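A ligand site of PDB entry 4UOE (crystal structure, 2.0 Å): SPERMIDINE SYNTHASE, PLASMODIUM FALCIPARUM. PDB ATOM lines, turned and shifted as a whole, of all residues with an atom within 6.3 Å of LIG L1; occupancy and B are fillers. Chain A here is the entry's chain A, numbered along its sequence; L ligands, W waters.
An oxygen (O2) of LIG L1 sits at hydrogen-bond distance from the side-chain carboxylate (OE2) of Glu 107 (2.7 Å). The side-chain carboxylate (OD1) of Asp 138 lies within hydrogen-bond range of a nitrogen (N3) of LIG L1 (2.8 Å). NE2 of Gln 32 lies within hydrogen-bond range of O2 of LIG L1 (3.0 Å). N2 of LIG L1 lies within hydrogen-bond range of N of Ala 164. N of Ala 139 sits at hydrogen-bond distance from N4 of LIG L1 (3.0 Å). O of Pro 163 sits at hydrogen-bond distance from N3 of LIG L1 (3.3 Å). The backbone NH (N) of Ile 108 is in hydrogen-bond range of a nitrogen (N5) of LIG L1 (3.3 Å). The side-chain hydroxyl (OG1) of Thr 166 sits at hydrogen-bond distance from a nitrogen (N3) of LIG L1, at 3.4 Å. The backbone NH (N) of Gly 85 sits close to a sulfur (S1) of LIG L1. The side-chain carboxylate (OD1) of Asp 156 is in salt-bridge range of a nitrogen (N1) of LG2 L2 (2.9 Å). O of Ser 157 is in hydrogen-bond range of N1 of LG2 L2 (2.7 Å).
S1 of LIG L1 lies close to N1 of LG2 L2 (3.8 Å).
The backbone NH of Gly 86 sits at hydrogen-bond distance from the side-chain carboxylate of Glu 107 (2.8 Å). OD1 of Asp 138 sits at hydrogen-bond distance from OG1 of Thr 166 (3.1 Å). The side-chain carboxylate of Asp 138 lies within hydrogen-bond range of the backbone NH of Ser 140, 2.9 Å away. NE2 of Gln 32 lies within hydrogen-bond range of OD2 of Asp 109 (3.1 Å). The backbone NH (N) of Asp 156 is in hydrogen-bond range of the backbone carbonyl oxygen (O) of Val 83 (2.7 Å). The backbone NH (N) of Gln 53 lies within hydrogen-bond range of the backbone carbonyl oxygen (O) of Leu 46 (2.8 Å). O of Cys 106 sits at hydrogen-bond distance from N of Gly 84, 2.9 Å away. O of Glu 137 is in hydrogen-bond range of SG of Cys 106 (3.2 Å).
The side-chain carboxylate (OD1) of Asp 87 sits close to a sulfur (S1) of LIG L1 (3.4 Å). The backbone carbonyl oxygen (O) of Asp 156 sits close to a sulfur (S1) of LIG L1 (3.6 Å). Leu 48 touches LIG L1 (CD1 to C5, 3.8 Å). Gln 53 touches LIG L1 (NE2 to C1, 3.4 Å). Gly 84 touches LIG L1. Cys 106 touches LIG L1. Asp 109 touches LIG L1 (CB to O2, 3.7 Å). CG1 of Val 112 touches O3 of LIG L1, at 3.5 Å. Glu 137 touches LIG L1 (O to C10, 3.9 Å). Ser 157 touches LIG L1 (C to C2, 3.6 Å). OG of Ser 158 touches C7 of LIG L1, 3.3 Å away. Leu 167 touches LIG L1. Hydrophobic or aromatic side chains that line LIG L1: Leu 48, Ile 108, Val 112, Ala 139, Pro 163, Ala 164 and Leu 167. Within 4 Å of LIG L1: Gln 32, Leu 48, Gln 53, Gly 84, Gly 85, Asp 87, Cys 106, Glu 107, Ile 108, Asp 109, Val 112, Glu 137, Asp 138, Ala 139, Asp 156, Ser 157, Ser 158, Pro 163, Ala 164, Thr 166 and Leu 167.
Water W1 lies within hydrogen-bond range of O of Gln 53, N1 of LG2 L2 and S1 of LIG L1.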
ATOM      1  N   TYR A  31      -5.758  -3.544  -8.511  1.00  0.00           N
ATOM      2  CA  TYR A  31      -4.781  -4.536  -8.966  1.00  0.00           C
ATOM      3  C   TYR A  31      -5.409  -5.525  -9.917  1.00  0.00           C
ATOM      4  O   TYR A  31      -4.709  -6.004 -10.779  1.00  0.00           O
ATOM      5  CB  TYR A  31      -4.073  -5.246  -7.778  1.00  0.00           C
ATOM      6  CG  TYR A  31      -3.214  -4.279  -7.018  1.00  0.00           C
ATOM      7  CD1 TYR A  31      -1.949  -3.910  -7.488  1.00  0.00           C
ATOM      8  CD2 TYR A  31      -3.697  -3.674  -5.870  1.00  0.00           C
ATOM      9  CE1 TYR A  31      -1.166  -2.968  -6.787  1.00  0.00           C
ATOM     10  CE2 TYR A  31      -2.930  -2.747  -5.168  1.00  0.00           C
ATOM     11  CZ  TYR A  31      -1.678  -2.421  -5.628  1.00  0.00           C
ATOM     12  OH  TYR A  31      -0.966  -1.509  -4.937  1.00  0.00           O
ATOM     13  N   GLN A  32      -6.695  -5.834  -9.787  1.00  0.00           N
ATOM     14  CA  GLN A  32      -7.167  -6.929 -10.541  1.00  0.00           C
ATOM     15  C   GLN A  32      -8.688  -6.989 -10.677  1.00  0.00           C
ATOM     16  O   GLN A  32      -9.429  -6.259 -10.027  1.00  0.00           O
ATOM     17  CB  GLN A  32      -6.485  -8.211  -9.973  1.00  0.00           C
ATOM     18  CG  GLN A  32      -6.955  -8.873  -8.706  1.00  0.00           C
ATOM     19  CD  GLN A  32      -5.803  -9.512  -7.830  1.00  0.00           C
ATOM     20  OE1 GLN A  32      -5.046 -10.454  -8.202  1.00  0.00           O
ATOM     21  NE2 GLN A  32      -5.702  -8.992  -6.613  1.00  0.00           N
ATOM     22  N   LEU A  46     -14.575 -17.528  -5.719  1.00  0.00           N
ATOM     23  CA  LEU A  46     -13.903 -16.238  -5.831  1.00  0.00           C
ATOM     24  C   LEU A  46     -12.979 -16.345  -6.977  1.00  0.00           C
ATOM     25  O   LEU A  46     -12.182 -17.277  -7.003  1.00  0.00           O
ATOM     26  CB  LEU A  46     -13.078 -15.963  -4.555  1.00  0.00           C
ATOM     27  CG  LEU A  46     -12.012 -14.804  -4.625  1.00  0.00           C
ATOM     28  CD1 LEU A  46     -12.726 -13.482  -4.754  1.00  0.00           C
ATOM     29  CD2 LEU A  46     -11.146 -14.698  -3.401  1.00  0.00           C
ATOM     30  N   LEU A  48     -10.194 -14.044  -9.594  1.00  0.00           N
ATOM     31  CA  LEU A  48      -9.318 -12.869  -9.704  1.00  0.00           C
ATOM     32  C   LEU A  48      -8.610 -13.023 -11.019  1.00  0.00           C
ATOM     33  O   LEU A  48      -7.960 -14.023 -11.257  1.00  0.00           O
ATOM     34  CB  LEU A  48      -8.269 -12.822  -8.584  1.00  0.00           C
ATOM     35  CG  LEU A  48      -8.767 -12.692  -7.163  1.00  0.00           C
ATOM     36  CD1 LEU A  48      -7.666 -12.794  -6.060  1.00  0.00           C
ATOM     37  CD2 LEU A  48      -9.425 -11.345  -7.051  1.00  0.00           C
ATOM     38  N   GLN A  53      -9.818 -18.784  -7.425  1.00  0.00           N
ATOM     39  CA  GLN A  53      -8.927 -18.753  -6.261  1.00  0.00           C
ATOM     40  C   GLN A  53      -9.421 -19.677  -5.197  1.00  0.00           C
ATOM     41  O   GLN A  53      -8.644 -20.271  -4.486  1.00  0.00           O
ATOM     42  CB  GLN A  53      -8.809 -17.335  -5.665  1.00  0.00           C
ATOM     43  CG  GLN A  53      -8.451 -16.289  -6.678  1.00  0.00           C
ATOM     44  CD  GLN A  53      -7.002 -16.341  -7.145  1.00  0.00           C
ATOM     45  OE1 GLN A  53      -6.713 -16.324  -8.363  1.00  0.00           O
ATOM     46  NE2 GLN A  53      -6.094 -16.320  -6.195  1.00  0.00           N
ATOM     47  N   LEU A  54     -10.718 -19.788  -5.048  1.00  0.00           N
ATOM     48  CA  LEU A  54     -11.242 -20.800  -4.171  1.00  0.00           C
ATOM     49  C   LEU A  54     -12.664 -21.070  -4.466  1.00  0.00           C
ATOM     50  O   LEU A  54     -13.299 -20.290  -5.142  1.00  0.00           O
ATOM     51  CB  LEU A  54     -11.102 -20.379  -2.702  1.00  0.00           C
ATOM     52  CG  LEU A  54     -11.858 -19.125  -2.177  1.00  0.00           C
ATOM     53  CD1 LEU A  54     -13.314 -19.352  -1.775  1.00  0.00           C
ATOM     54  CD2 LEU A  54     -11.078 -18.591  -0.987  1.00  0.00           C
ATOM     55  N   VAL A  83       1.697 -14.398   3.332  1.00  0.00           N
ATOM     56  CA  VAL A  83       1.721 -13.570   2.106  1.00  0.00           C
ATOM     57  C   VAL A  83       0.542 -13.911   1.204  1.00  0.00           C
ATOM     58  O   VAL A  83       0.263 -15.087   0.915  1.00  0.00           O
ATOM     59  CB  VAL A  83       2.992 -13.765   1.310  1.00  0.00           C
ATOM     60  CG1 VAL A  83       2.879 -13.079  -0.056  1.00  0.00           C
ATOM     61  CG2 VAL A  83       4.192 -13.301   2.121  1.00  0.00           C
ATOM     62  N   GLY A  84      -0.159 -12.873   0.740  1.00  0.00           N
ATOM     63  CA  GLY A  84      -1.337 -13.089  -0.041  1.00  0.00           C
ATOM     64  C   GLY A  84      -2.426 -13.541   0.890  1.00  0.00           C
ATOM     65  O   GLY A  84      -2.526 -13.071   1.997  1.00  0.00           O
ATOM     66  N   GLY A  85      -3.252 -14.464   0.491  1.00  0.00           N
ATOM     67  CA  GLY A  85      -4.238 -14.996   1.399  1.00  0.00           C
ATOM     68  C   GLY A  85      -5.360 -14.092   1.924  1.00  0.00           C
ATOM     69  O   GLY A  85      -5.910 -14.404   3.021  1.00  0.00           O
ATOM     70  N   GLY A  86      -5.736 -13.061   1.144  1.00  0.00           N
ATOM     71  CA  GLY A  86      -6.779 -12.105   1.522  1.00  0.00           C
ATOM     72  C   GLY A  86      -8.073 -12.812   1.931  1.00  0.00           C
ATOM     73  O   GLY A  86      -8.856 -12.341   2.767  1.00  0.00           O
ATOM     74  N   ASP A  87      -8.334 -13.963   1.349  1.00  0.00           N
ATOM     75  CA  ASP A  87      -9.597 -14.654   1.729  1.00  0.00           C
ATOM     76  C   ASP A  87      -9.639 -14.958   3.203  1.00  0.00           C
ATOM     77  O   ASP A  87     -10.726 -15.118   3.798  1.00  0.00           O
ATOM     78  CB  ASP A  87      -9.775 -15.934   0.940  1.00  0.00           C
ATOM     79  CG  ASP A  87      -8.543 -16.774   0.922  1.00  0.00           C
ATOM     80  OD1 ASP A  87      -7.651 -16.525   0.063  1.00  0.00           O
ATOM     81  OD2 ASP A  87      -8.448 -17.627   1.810  1.00  0.00           O
ATOM     82  N   CYS A 106       0.203  -9.946   4.910  1.00  0.00           N
ATOM     83  CA  CYS A 106       0.494  -8.971   3.900  1.00  0.00           C
ATOM     84  C   CYS A 106      -0.183  -9.326   2.532  1.00  0.00           C
ATOM     85  O   CYS A 106       0.239 -10.249   1.825  1.00  0.00           O
ATOM     86  CB  CYS A 106       1.968  -8.839   3.770  1.00  0.00           C
ATOM     87  SG  CYS A 106       2.401  -7.531   2.620  1.00  0.00           S
ATOM     88  N   GLU A 107      -1.246  -8.585   2.222  1.00  0.00           N
ATOM     89  CA  GLU A 107      -2.088  -8.738   1.033  1.00  0.00           C
ATOM     90  C   GLU A 107      -2.110  -7.414   0.266  1.00  0.00           C
ATOM     91  O   GLU A 107      -2.285  -6.312   0.858  1.00  0.00           O
ATOM     92  CB  GLU A 107      -3.476  -9.083   1.515  1.00  0.00           C
ATOM     93  CG  GLU A 107      -4.625  -8.955   0.517  1.00  0.00           C
ATOM     94  CD  GLU A 107      -4.530  -9.873  -0.676  1.00  0.00           C
ATOM     95  OE1 GLU A 107      -4.644 -11.156  -0.525  1.00  0.00           O
ATOM     96  OE2 GLU A 107      -4.339  -9.282  -1.752  1.00  0.00           O
ATOM     97  N   ILE A 108      -1.942  -7.508  -1.038  1.00  0.00           N
ATOM     98  CA  ILE A 108      -1.701  -6.305  -1.841  1.00  0.00           C
ATOM     99  C   ILE A 108      -3.045  -5.620  -2.111  1.00  0.00           C
ATOM    100  O   ILE A 108      -3.117  -4.392  -2.195  1.00  0.00           O
ATOM    101  CB  ILE A 108      -0.895  -6.612  -3.124  1.00  0.00           C
ATOM    102  CG1 ILE A 108      -0.301  -5.339  -3.721  1.00  0.00           C
ATOM    103  CG2 ILE A 108      -1.738  -7.319  -4.183  1.00  0.00           C
ATOM    104  CD1 ILE A 108       0.501  -5.607  -4.973  1.00  0.00           C
ATOM    105  N   ASP A 109      -4.099  -6.406  -2.135  1.00  0.00           N
ATOM    106  CA  ASP A 109      -5.409  -5.934  -2.558  1.00  0.00           C
ATOM    107  C   ASP A 109      -6.491  -6.013  -1.494  1.00  0.00           C
ATOM    108  O   ASP A 109      -7.156  -7.054  -1.368  1.00  0.00           O
ATOM    109  CB  ASP A 109      -5.850  -6.768  -3.785  1.00  0.00           C
ATOM    110  CG  ASP A 109      -7.055  -6.158  -4.521  1.00  0.00           C
ATOM    111  OD1 ASP A 109      -7.834  -5.375  -3.906  1.00  0.00           O
ATOM    112  OD2 ASP A 109      -7.194  -6.455  -5.722  1.00  0.00           O
ATOM    113  N   VAL A 112      -9.963  -7.775  -1.810  1.00  0.00           N
ATOM    114  CA  VAL A 112     -10.079  -9.237  -1.565  1.00  0.00           C
ATOM    115  C   VAL A 112     -10.524  -9.539  -0.115  1.00  0.00           C
ATOM    116  O   VAL A 112     -11.508 -10.273   0.139  1.00  0.00           O
ATOM    117  CB  VAL A 112      -8.771  -9.966  -1.949  1.00  0.00           C
ATOM    118  CG1 VAL A 112      -8.923 -11.453  -1.605  1.00  0.00           C
ATOM    119  CG2 VAL A 112      -8.478  -9.825  -3.422  1.00  0.00           C
ATOM    120  N   GLU A 137      -0.123  -4.054   1.227  1.00  0.00           N
ATOM    121  CA  GLU A 137       1.135  -3.728   0.570  1.00  0.00           C
ATOM    122  C   GLU A 137       1.598  -4.913  -0.259  1.00  0.00           C
ATOM    123  O   GLU A 137       1.222  -6.074   0.003  1.00  0.00           O
ATOM    124  CB  GLU A 137       2.171  -3.422   1.666  1.00  0.00           C
ATOM    125  CG  GLU A 137       3.394  -2.666   1.217  1.00  0.00           C
ATOM    126  CD  GLU A 137       4.505  -2.622   2.285  1.00  0.00           C
ATOM    127  OE1 GLU A 137       4.286  -2.971   3.485  1.00  0.00           O
ATOM    128  OE2 GLU A 137       5.618  -2.227   1.900  1.00  0.00           O
ATOM    129  N   ASP A 138       2.339  -4.630  -1.311  1.00  0.00           N
ATOM    130  CA  ASP A 138       3.073  -5.626  -2.030  1.00  0.00           C
ATOM    131  C   ASP A 138       4.042  -6.347  -1.079  1.00  0.00           C
ATOM    132  O   ASP A 138       4.932  -5.708  -0.509  1.00  0.00           O
ATOM    133  CB  ASP A 138       3.906  -4.968  -3.167  1.00  0.00           C
ATOM    134  CG  ASP A 138       4.486  -5.998  -4.155  1.00  0.00           C
ATOM    135  OD1 ASP A 138       4.739  -7.185  -3.789  1.00  0.00           O
ATOM    136  OD2 ASP A 138       4.748  -5.626  -5.314  1.00  0.00           O
ATOM    137  N   ALA A 139       3.946  -7.671  -0.973  1.00  0.00           N
ATOM    138  CA  ALA A 139       4.795  -8.395  -0.044  1.00  0.00           C
ATOM    139  C   ALA A 139       6.262  -8.304  -0.435  1.00  0.00           C
ATOM    140  O   ALA A 139       7.110  -8.430   0.411  1.00  0.00           O
ATOM    141  CB  ALA A 139       4.367  -9.831   0.104  1.00  0.00           C
ATOM    142  N   SER A 140       6.552  -8.078  -1.695  1.00  0.00           N
ATOM    143  CA  SER A 140       7.941  -7.844  -2.081  1.00  0.00           C
ATOM    144  C   SER A 140       8.552  -6.645  -1.365  1.00  0.00           C
ATOM    145  O   SER A 140       9.765  -6.648  -1.053  1.00  0.00           O
ATOM    146  CB  SER A 140       8.096  -7.645  -3.591  1.00  0.00           C
ATOM    147  OG  SER A 140       9.428  -7.258  -3.894  1.00  0.00           O
ATOM    148  N   ASP A 156       0.586 -17.703   0.270  1.00  0.00           N
ATOM    149  CA  ASP A 156      -0.649 -18.035  -0.386  1.00  0.00           C
ATOM    150  C   ASP A 156      -0.920 -17.008  -1.507  1.00  0.00           C
ATOM    151  O   ASP A 156      -1.815 -16.208  -1.423  1.00  0.00           O
ATOM    152  CB  ASP A 156      -1.791 -18.091   0.596  1.00  0.00           C
ATOM    153  CG  ASP A 156      -3.088 -18.405  -0.056  1.00  0.00           C
ATOM    154  OD1 ASP A 156      -3.093 -18.734  -1.257  1.00  0.00           O
ATOM    155  OD2 ASP A 156      -4.106 -18.285   0.611  1.00  0.00           O
ATOM    156  N   SER A 157      -0.115 -17.071  -2.567  1.00  0.00           N
ATOM    157  CA  SER A 157      -0.264 -16.194  -3.705  1.00  0.00           C
ATOM    158  C   SER A 157      -1.231 -16.676  -4.794  1.00  0.00           C
ATOM    159  O   SER A 157      -1.592 -17.831  -4.911  1.00  0.00           O
ATOM    160  CB  SER A 157       1.068 -16.002  -4.387  1.00  0.00           C
ATOM    161  OG  SER A 157       1.442 -17.163  -5.110  1.00  0.00           O
ATOM    162  N   SER A 158      -1.619 -15.717  -5.587  1.00  0.00           N
ATOM    163  CA  SER A 158      -2.200 -15.979  -6.890  1.00  0.00           C
ATOM    164  C   SER A 158      -1.026 -16.361  -7.863  1.00  0.00           C
ATOM    165  O   SER A 158       0.154 -16.353  -7.457  1.00  0.00           O
ATOM    166  CB  SER A 158      -2.972 -14.718  -7.357  1.00  0.00           C
ATOM    167  OG  SER A 158      -2.138 -13.569  -7.171  1.00  0.00           O
ATOM    168  N   GLY A 162      -0.097 -11.164 -13.243  1.00  0.00           N
ATOM    169  CA  GLY A 162      -0.756 -10.275 -12.307  1.00  0.00           C
ATOM    170  C   GLY A 162       0.150  -9.773 -11.183  1.00  0.00           C
ATOM    171  O   GLY A 162       1.361  -9.646 -11.353  1.00  0.00           O
ATOM    172  N   PRO A 163      -0.450  -9.432 -10.043  1.00  0.00           N
ATOM    173  CA  PRO A 163       0.325  -8.734  -8.995  1.00  0.00           C
ATOM    174  C   PRO A 163       1.316  -9.643  -8.258  1.00  0.00           C
ATOM    175  O   PRO A 163       2.312  -9.153  -7.722  1.00  0.00           O
ATOM    176  CB  PRO A 163      -0.740  -8.179  -8.046  1.00  0.00           C
ATOM    177  CG  PRO A 163      -2.045  -8.845  -8.414  1.00  0.00           C
ATOM    178  CD  PRO A 163      -1.917  -9.395  -9.795  1.00  0.00           C
ATOM    179  N   ALA A 164       1.073 -10.941  -8.295  1.00  0.00           N
ATOM    180  CA  ALA A 164       1.988 -11.903  -7.786  1.00  0.00           C
ATOM    181  C   ALA A 164       3.229 -12.109  -8.611  1.00  0.00           C
ATOM    182  O   ALA A 164       4.062 -12.886  -8.226  1.00  0.00           O
ATOM    183  CB  ALA A 164       1.312 -13.234  -7.538  1.00  0.00           C
ATOM    184  N   GLU A 165       3.401 -11.399  -9.702  1.00  0.00           N
ATOM    185  CA  GLU A 165       4.612 -11.572 -10.507  1.00  0.00           C
ATOM    186  C   GLU A 165       5.874 -11.267  -9.700  1.00  0.00           C
ATOM    187  O   GLU A 165       6.907 -11.803 -10.031  1.00  0.00           O
ATOM    188  CB  GLU A 165       4.573 -10.710 -11.775  1.00  0.00           C
ATOM    189  CG  GLU A 165       4.676  -9.206 -11.577  1.00  0.00           C
ATOM    190  CD  GLU A 165       4.154  -8.439 -12.802  1.00  0.00           C
ATOM    191  OE1 GLU A 165       4.520  -8.819 -13.958  1.00  0.00           O
ATOM    192  OE2 GLU A 165       3.331  -7.498 -12.615  1.00  0.00           O
ATOM    193  N   THR A 166       5.803 -10.425  -8.671  1.00  0.00           N
ATOM    194  CA  THR A 166       6.979 -10.103  -7.854  1.00  0.00           C
ATOM    195  C   THR A 166       7.324 -11.201  -6.846  1.00  0.00           C
ATOM    196  O   THR A 166       8.297 -11.091  -6.137  1.00  0.00           O
ATOM    197  CB  THR A 166       6.794  -8.758  -7.092  1.00  0.00           C
ATOM    198  OG1 THR A 166       5.612  -8.812  -6.239  1.00  0.00           O
ATOM    199  CG2 THR A 166       6.658  -7.638  -8.063  1.00  0.00           C
ATOM    200  N   LEU A 167       6.486 -12.223  -6.728  1.00  0.00           N
ATOM    201  CA  LEU A 167       6.695 -13.259  -5.771  1.00  0.00           C
ATOM    202  C   LEU A 167       7.315 -14.594  -6.303  1.00  0.00           C
ATOM    203  O   LEU A 167       7.449 -15.554  -5.541  1.00  0.00           O
ATOM    204  CB  LEU A 167       5.370 -13.576  -5.111  1.00  0.00           C
ATOM    205  CG  LEU A 167       4.579 -12.390  -4.608  1.00  0.00           C
ATOM    206  CD1 LEU A 167       3.414 -12.929  -3.796  1.00  0.00           C
ATOM    207  CD2 LEU A 167       5.442 -11.450  -3.767  1.00  0.00           C
HETATM  208  C1  LIG L   1      -6.643 -15.103  -3.077  1.00  0.00           C
HETATM  209  S1  LIG L   1      -5.283 -15.754  -2.201  1.00  0.00           S
HETATM  210  C2  LIG L   1      -4.024 -15.039  -3.244  1.00  0.00           C
HETATM  211  C3  LIG L   1      -3.835 -13.552  -2.981  1.00  0.00           C
HETATM  212  O1  LIG L   1      -2.563 -13.124  -3.427  1.00  0.00           O
HETATM  213  C4  LIG L   1      -3.742 -11.470  -4.267  1.00  0.00           C
HETATM  214  O2  LIG L   1      -4.242 -10.121  -4.268  1.00  0.00           O
HETATM  215  C5  LIG L   1      -4.689 -12.528  -3.746  1.00  0.00           C
HETATM  216  O3  LIG L   1      -5.673 -12.049  -2.873  1.00  0.00           O
HETATM  217  C6  LIG L   1      -2.548 -11.695  -3.405  1.00  0.00           C
HETATM  218  N1  LIG L   1      -1.339 -11.154  -3.999  1.00  0.00           N
HETATM  219  C7  LIG L   1      -0.918 -11.172  -5.247  1.00  0.00           C
HETATM  220  N2  LIG L   1       0.276 -10.526  -5.411  1.00  0.00           N
HETATM  221  C8  LIG L   1       0.642 -10.139  -4.197  1.00  0.00           C
HETATM  222  C9  LIG L   1       1.742  -9.397  -3.664  1.00  0.00           C
HETATM  223  N3  LIG L   1       2.774  -9.029  -4.462  1.00  0.00           N
HETATM  224  N4  LIG L   1       1.730  -9.212  -2.348  1.00  0.00           N
HETATM  225  C10 LIG L   1       0.730  -9.580  -1.531  1.00  0.00           C
HETATM  226  N5  LIG L   1      -0.341 -10.235  -1.979  1.00  0.00           N
HETATM  227  C11 LIG L   1      -0.435 -10.522  -3.283  1.00  0.00           C
HETATM  228  N1  LG2 L   2      -3.946 -18.783  -3.978  1.00  0.00           N
HETATM  229  C1  LG2 L   2      -4.086 -20.170  -4.341  1.00  0.00           C
HETATM  230  C2  LG2 L   2      -4.119 -20.423  -5.849  1.00  0.00           C
HETATM  231  C3  LG2 L   2      -4.696 -19.477  -6.704  1.00  0.00           C
HETATM  232  C4  LG2 L   2      -4.720 -19.683  -8.082  1.00  0.00           C
HETATM  233  C5  LG2 L   2      -4.231 -20.870  -8.650  1.00  0.00           C
HETATM  234  C6  LG2 L   2      -3.672 -21.837  -7.810  1.00  0.00           C
HETATM  235  C7  LG2 L   2      -3.629 -21.624  -6.414  1.00  0.00           C
HETATM  236  N2  LG2 L   2      -4.296 -21.018  -9.996  1.00  0.00           N
HETATM  237  O   HOH W   1      -6.727 -18.597  -3.274  1.00  0.00           O
